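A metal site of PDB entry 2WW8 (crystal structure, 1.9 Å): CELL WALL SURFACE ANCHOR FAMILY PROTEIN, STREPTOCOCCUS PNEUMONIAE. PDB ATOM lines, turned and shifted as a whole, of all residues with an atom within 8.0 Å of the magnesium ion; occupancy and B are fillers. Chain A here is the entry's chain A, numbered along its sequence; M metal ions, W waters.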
ATOM      1  N   ASP A 232      21.541  21.574  20.837  1.00  0.00           N
ATOM      2  CA  ASP A 232      22.357  22.610  21.501  1.00  0.00           C
ATOM      3  C   ASP A 232      23.526  21.956  22.266  1.00  0.00           C
ATOM      4  O   ASP A 232      23.352  21.059  23.101  1.00  0.00           O
ATOM      5  CB  ASP A 232      21.354  23.453  22.355  1.00  0.00           C
ATOM      6  CG  ASP A 232      21.978  24.582  23.194  1.00  0.00           C
ATOM      7  OD1 ASP A 232      23.206  24.613  23.444  1.00  0.00           O
ATOM      8  OD2 ASP A 232      21.120  25.427  23.583  1.00  0.00           O
ATOM      9  N   ASN A 233      24.751  22.378  21.932  1.00  0.00           N
ATOM     10  CA  ASN A 233      25.950  21.883  22.650  1.00  0.00           C
ATOM     11  C   ASN A 233      26.687  23.112  23.273  1.00  0.00           C
ATOM     12  O   ASN A 233      27.925  23.098  23.374  1.00  0.00           O
ATOM     13  CB  ASN A 233      26.862  21.073  21.718  1.00  0.00           C
ATOM     14  CG  ASN A 233      27.950  20.256  22.453  1.00  0.00           C
ATOM     15  OD1 ASN A 233      29.111  20.394  22.095  1.00  0.00           O
ATOM     16  ND2 ASN A 233      27.615  19.480  23.462  1.00  0.00           N
ATOM     17  N   SER A 234      25.943  24.147  23.658  1.00  0.00           N
ATOM     18  CA  SER A 234      26.514  25.359  24.275  1.00  0.00           C
ATOM     19  C   SER A 234      27.159  24.974  25.652  1.00  0.00           C
ATOM     20  O   SER A 234      26.880  23.909  26.227  1.00  0.00           O
ATOM     21  CB  SER A 234      25.455  26.471  24.428  1.00  0.00           C
ATOM     22  OG  SER A 234      24.429  25.956  25.282  1.00  0.00           O
ATOM     23  N   ASN A 235      28.022  25.847  26.199  1.00  0.00           N
ATOM     24  CA  ASN A 235      28.768  25.546  27.429  1.00  0.00           C
ATOM     25  C   ASN A 235      27.863  25.176  28.611  1.00  0.00           C
ATOM     26  O   ASN A 235      28.196  24.295  29.393  1.00  0.00           O
ATOM     27  CB  ASN A 235      29.583  26.795  27.802  1.00  0.00           C
ATOM     28  CG  ASN A 235      30.654  27.130  26.765  1.00  0.00           C
ATOM     29  OD1 ASN A 235      31.100  26.249  26.028  1.00  0.00           O
ATOM     30  ND2 ASN A 235      31.024  28.391  26.686  1.00  0.00           N
ATOM     31  N   SER A 236      26.718  25.870  28.753  1.00  0.00           N
ATOM     32  CA  SER A 236      25.738  25.593  29.799  1.00  0.00           C
ATOM     33  C   SER A 236      25.261  24.136  29.791  1.00  0.00           C
ATOM     34  O   SER A 236      24.687  23.674  30.771  1.00  0.00           O
ATOM     35  CB  SER A 236      24.494  26.457  29.580  1.00  0.00           C
ATOM     36  OG  SER A 236      23.886  26.211  28.310  1.00  0.00           O
ATOM     37  N   MET A 237      25.432  23.423  28.659  1.00  0.00           N
ATOM     38  CA  MET A 237      25.048  21.988  28.667  1.00  0.00           C
ATOM     39  C   MET A 237      26.037  21.094  29.407  1.00  0.00           C
ATOM     40  O   MET A 237      25.753  19.942  29.630  1.00  0.00           O
ATOM     41  CB  MET A 237      24.857  21.439  27.232  1.00  0.00           C
ATOM     42  CG  MET A 237      23.780  22.170  26.410  1.00  0.00           C
ATOM     43  SD  MET A 237      22.161  21.601  26.970  1.00  0.00           S
ATOM     44  CE  MET A 237      22.070  19.952  26.283  1.00  0.00           C
ATOM     45  N   SER A 238      27.241  21.586  29.718  1.00  0.00           N
ATOM     46  CA  SER A 238      28.222  20.841  30.492  1.00  0.00           C
ATOM     47  C   SER A 238      27.632  20.056  31.666  1.00  0.00           C
ATOM     48  O   SER A 238      26.850  20.601  32.460  1.00  0.00           O
ATOM     49  CB  SER A 238      29.228  21.869  31.053  1.00  0.00           C
ATOM     50  OG  SER A 238      29.943  21.284  32.115  1.00  0.00           O
ATOM     51  N   ASN A 242      24.902  23.489  36.410  1.00  0.00           N
ATOM     52  CA  ASN A 242      23.484  23.482  36.777  1.00  0.00           C
ATOM     53  C   ASN A 242      23.202  22.508  37.915  1.00  0.00           C
ATOM     54  O   ASN A 242      22.197  21.772  37.842  1.00  0.00           O
ATOM     55  CB  ASN A 242      22.591  23.185  35.561  1.00  0.00           C
ATOM     56  CG  ASN A 242      23.048  23.958  34.346  1.00  0.00           C
ATOM     57  OD1 ASN A 242      22.969  25.182  34.338  1.00  0.00           O
ATOM     58  ND2 ASN A 242      23.531  23.266  33.310  1.00  0.00           N
ATOM     59  N   ARG A 247      23.170  17.791  31.690  1.00  0.00           N
ATOM     60  CA  ARG A 247      22.411  18.171  30.525  1.00  0.00           C
ATOM     61  C   ARG A 247      22.870  17.495  29.228  1.00  0.00           C
ATOM     62  O   ARG A 247      22.035  16.885  28.512  1.00  0.00           O
ATOM     63  CB  ARG A 247      22.363  19.683  30.304  1.00  0.00           C
ATOM     64  CG  ARG A 247      21.521  20.402  31.397  1.00  0.00           C
ATOM     65  CD  ARG A 247      21.395  21.886  31.054  1.00  0.00           C
ATOM     66  NE  ARG A 247      20.642  22.573  32.096  1.00  0.00           N
ATOM     67  CZ  ARG A 247      20.488  23.889  32.115  1.00  0.00           C
ATOM     68  NH1 ARG A 247      21.074  24.657  31.193  1.00  0.00           N
ATOM     69  NH2 ARG A 247      19.800  24.427  33.109  1.00  0.00           N
ATOM     70  N   TYR A 275      25.004  22.372  17.441  1.00  0.00           N
ATOM     71  CA  TYR A 275      25.367  23.808  17.312  1.00  0.00           C
ATOM     72  C   TYR A 275      25.713  24.466  18.655  1.00  0.00           C
ATOM     73  O   TYR A 275      25.217  24.060  19.702  1.00  0.00           O
ATOM     74  CB  TYR A 275      24.292  24.669  16.650  1.00  0.00           C
ATOM     75  CG  TYR A 275      23.048  24.944  17.484  1.00  0.00           C
ATOM     76  CD1 TYR A 275      22.050  23.961  17.631  1.00  0.00           C
ATOM     77  CD2 TYR A 275      22.874  26.162  18.126  1.00  0.00           C
ATOM     78  CE1 TYR A 275      20.891  24.218  18.363  1.00  0.00           C
ATOM     79  CE2 TYR A 275      21.680  26.450  18.852  1.00  0.00           C
ATOM     80  CZ  TYR A 275      20.716  25.477  18.942  1.00  0.00           C
ATOM     81  OH  TYR A 275      19.611  25.760  19.728  1.00  0.00           O
ATOM     82  N   ALA A 276      26.476  25.547  18.549  1.00  0.00           N
ATOM     83  CA  ALA A 276      26.647  26.452  19.688  1.00  0.00           C
ATOM     84  C   ALA A 276      26.918  27.807  19.026  1.00  0.00           C
ATOM     85  O   ALA A 276      25.929  28.366  18.472  1.00  0.00           O
ATOM     86  CB  ALA A 276      27.704  25.962  20.730  1.00  0.00           C
ATOM     87  N   GLY A 355      31.191  28.288  22.489  1.00  0.00           N
ATOM     88  CA  GLY A 355      29.992  27.644  23.071  1.00  0.00           C
ATOM     89  C   GLY A 355      28.821  28.546  23.456  1.00  0.00           C
ATOM     90  O   GLY A 355      28.203  28.302  24.490  1.00  0.00           O
ATOM     91  N   ALA A 356      28.572  29.604  22.703  1.00  0.00           N
ATOM     92  CA  ALA A 356      27.392  30.441  22.892  1.00  0.00           C
ATOM     93  C   ALA A 356      26.200  29.807  22.087  1.00  0.00           C
ATOM     94  O   ALA A 356      26.300  28.662  21.666  1.00  0.00           O
ATOM     95  CB  ALA A 356      27.648  31.864  22.371  1.00  0.00           C
ATOM     96  N   THR A 357      25.143  30.556  21.803  1.00  0.00           N
ATOM     97  CA  THR A 357      23.866  30.030  21.314  1.00  0.00           C
ATOM     98  C   THR A 357      23.426  30.771  20.056  1.00  0.00           C
ATOM     99  O   THR A 357      22.721  31.790  20.129  1.00  0.00           O
ATOM    100  CB  THR A 357      22.816  30.058  22.430  1.00  0.00           C
ATOM    101  OG1 THR A 357      23.414  29.478  23.587  1.00  0.00           O
ATOM    102  CG2 THR A 357      21.514  29.244  22.043  1.00  0.00           C
ATOM    103  N   THR A 386      17.153  22.366  23.105  1.00  0.00           N
ATOM    104  CA  THR A 386      18.040  23.472  23.460  1.00  0.00           C
ATOM    105  C   THR A 386      17.945  23.803  24.960  1.00  0.00           C
ATOM    106  O   THR A 386      16.905  23.500  25.583  1.00  0.00           O
ATOM    107  CB  THR A 386      17.680  24.706  22.581  1.00  0.00           C
ATOM    108  OG1 THR A 386      18.354  25.872  23.064  1.00  0.00           O
ATOM    109  CG2 THR A 386      16.198  24.944  22.512  1.00  0.00           C
ATOM    110  N   ASP A 387      18.990  24.456  25.513  1.00  0.00           N
ATOM    111  CA  ASP A 387      18.867  24.906  26.913  1.00  0.00           C
ATOM    112  C   ASP A 387      19.016  26.427  27.022  1.00  0.00           C
ATOM    113  O   ASP A 387      19.350  26.944  28.067  1.00  0.00           O
ATOM    114  CB  ASP A 387      19.836  24.178  27.847  1.00  0.00           C
ATOM    115  CG  ASP A 387      21.233  24.751  27.753  1.00  0.00           C
ATOM    116  OD1 ASP A 387      21.575  25.431  26.766  1.00  0.00           O
ATOM    117  OD2 ASP A 387      22.056  24.444  28.623  1.00  0.00           O
ATOM    118  N   GLY A 388      18.790  27.151  25.933  1.00  0.00           N
ATOM    119  CA  GLY A 388      18.881  28.609  26.074  1.00  0.00           C
ATOM    120  C   GLY A 388      18.427  29.437  24.893  1.00  0.00           C
ATOM    121  O   GLY A 388      18.393  28.993  23.746  1.00  0.00           O
ATOM    122  N   VAL A 389      17.994  30.646  25.210  1.00  0.00           N
ATOM    123  CA  VAL A 389      17.635  31.634  24.217  1.00  0.00           C
ATOM    124  C   VAL A 389      18.847  32.104  23.411  1.00  0.00           C
ATOM    125  O   VAL A 389      19.970  31.997  23.904  1.00  0.00           O
ATOM    126  CB  VAL A 389      16.882  32.808  24.875  1.00  0.00           C
ATOM    127  CG1 VAL A 389      15.612  32.306  25.639  1.00  0.00           C
ATOM    128  CG2 VAL A 389      17.777  33.603  25.828  1.00  0.00           C
ATOM    129  N   THR A 391      21.848  34.178  21.657  1.00  0.00           N
ATOM    130  CA  THR A 391      22.716  35.201  22.146  1.00  0.00           C
ATOM    131  C   THR A 391      23.626  35.651  20.978  1.00  0.00           C
ATOM    132  O   THR A 391      24.574  36.407  21.197  1.00  0.00           O
ATOM    133  CB  THR A 391      23.577  34.746  23.350  1.00  0.00           C
ATOM    134  OG1 THR A 391      24.295  33.558  22.999  1.00  0.00           O
ATOM    135  CG2 THR A 391      22.757  34.499  24.666  1.00  0.00           C
ATOM    136  N   ILE A 539      15.496  22.853  27.878  1.00  0.00           N
ATOM    137  CA  ILE A 539      16.031  22.277  29.106  1.00  0.00           C
ATOM    138  C   ILE A 539      16.274  23.427  30.099  1.00  0.00           C
ATOM    139  O   ILE A 539      17.289  24.132  30.014  1.00  0.00           O
ATOM    140  CB  ILE A 539      17.320  21.513  28.865  1.00  0.00           C
ATOM    141  CG1 ILE A 539      17.069  20.316  27.937  1.00  0.00           C
ATOM    142  CG2 ILE A 539      17.834  20.961  30.211  1.00  0.00           C
ATOM    143  CD1 ILE A 539      18.347  19.977  27.183  1.00  0.00           C
ATOM    144  N   ILE A 541      14.903  26.250  30.550  1.00  0.00           N
ATOM    145  CA  ILE A 541      14.964  27.588  29.965  1.00  0.00           C
ATOM    146  C   ILE A 541      14.327  28.655  30.840  1.00  0.00           C
ATOM    147  O   ILE A 541      13.171  28.459  31.247  1.00  0.00           O
ATOM    148  CB  ILE A 541      14.239  27.673  28.592  1.00  0.00           C
ATOM    149  CG1 ILE A 541      14.761  26.520  27.761  1.00  0.00           C
ATOM    150  CG2 ILE A 541      14.423  29.077  27.883  1.00  0.00           C
ATOM    151  CD1 ILE A 541      15.819  26.761  26.822  1.00  0.00           C
ATOM    152  N   ASP A 544      18.035  33.381  30.870  1.00  0.00           N
ATOM    153  CA  ASP A 544      19.419  33.745  31.106  1.00  0.00           C
ATOM    154  C   ASP A 544      20.169  33.464  29.829  1.00  0.00           C
ATOM    155  O   ASP A 544      19.945  32.448  29.174  1.00  0.00           O
ATOM    156  CB  ASP A 544      20.019  32.862  32.220  1.00  0.00           C
ATOM    157  CG  ASP A 544      19.603  33.298  33.614  1.00  0.00           C
ATOM    158  OD1 ASP A 544      19.014  34.416  33.763  1.00  0.00           O
ATOM    159  OD2 ASP A 544      19.833  32.532  34.579  1.00  0.00           O
ATOM    160  N   PRO A 545      21.074  34.351  29.443  1.00  0.00           N
ATOM    161  CA  PRO A 545      21.293  35.664  30.032  1.00  0.00           C
ATOM    162  C   PRO A 545      20.519  36.767  29.290  1.00  0.00           C
ATOM    163  O   PRO A 545      20.527  36.783  28.045  1.00  0.00           O
ATOM    164  CB  PRO A 545      22.810  35.850  29.797  1.00  0.00           C
ATOM    165  CG  PRO A 545      23.043  35.120  28.474  1.00  0.00           C
ATOM    166  CD  PRO A 545      22.065  33.998  28.408  1.00  0.00           C
HETATM  167 MG    MG M   1      23.010  27.066  26.506  1.00  0.00          MG
HETATM  168  O   HOH W   1      24.272  28.646  26.643  1.00  0.00           O
HETATM  169  O   HOH W   2      21.964  27.596  24.786  1.00  0.00           O
HETATM  170  O   HOH W   3      21.858  28.054  27.956  1.00  0.00           O
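The backbone NH (N) of Asp 387 lies within hydrogen-bond range of the side-chain carboxylate (OD2) of Asp 232 (3.0 Å). OD2 of Asp 232 is in hydrogen-bond range of OG1 of Thr 386 (2.8 Å). OD2 of Asp 387 is in salt-bridge range of NH1 of Arg 247 (2.8 Å). The backbone carbonyl oxygen (O) of Thr 357 lies within hydrogen-bond range of the backbone NH (N) of Thr 391 (3.0 Å). The backbone NH of Ser 234 is in hydrogen-bond range of the side-chain carboxylate of Asp 232 (2.8 Å). ND2 of Asn 242 is in hydrogen-bond range of O of Ser 236, 2.8 Å away.
Asp 232 touches the magnesium ion (OD2 to MG, 3.8 Å). Thr 357 touches the magnesium ion (OG1 to MG, 3.8 Å). Within 4 Å of the magnesium ion: Asp 232, Ser 234, Ser 236, Thr 357 and Asp 387. Along chain A the residues within 4 Å of the magnesium ion span positions 232 to 387. The nearest printed residue that does not touch the magnesium ion is Gly 388 (4.3 Å).
The magnesium ion is bound by water W1 (2.0 Å), water W2 (2.1 Å), water W3 (2.1 Å), OG of Ser 234 (2.2 Å), OG of Ser 236 (2.2 Å) and OD1 of Asp 387 (2.2 Å).
Water W2 lies within hydrogen-bond range of OD2 of Asp 232 (2.6 Å), OG1 of Thr 357 (2.7 Å) and N of Gly 388 (3.4 Å).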
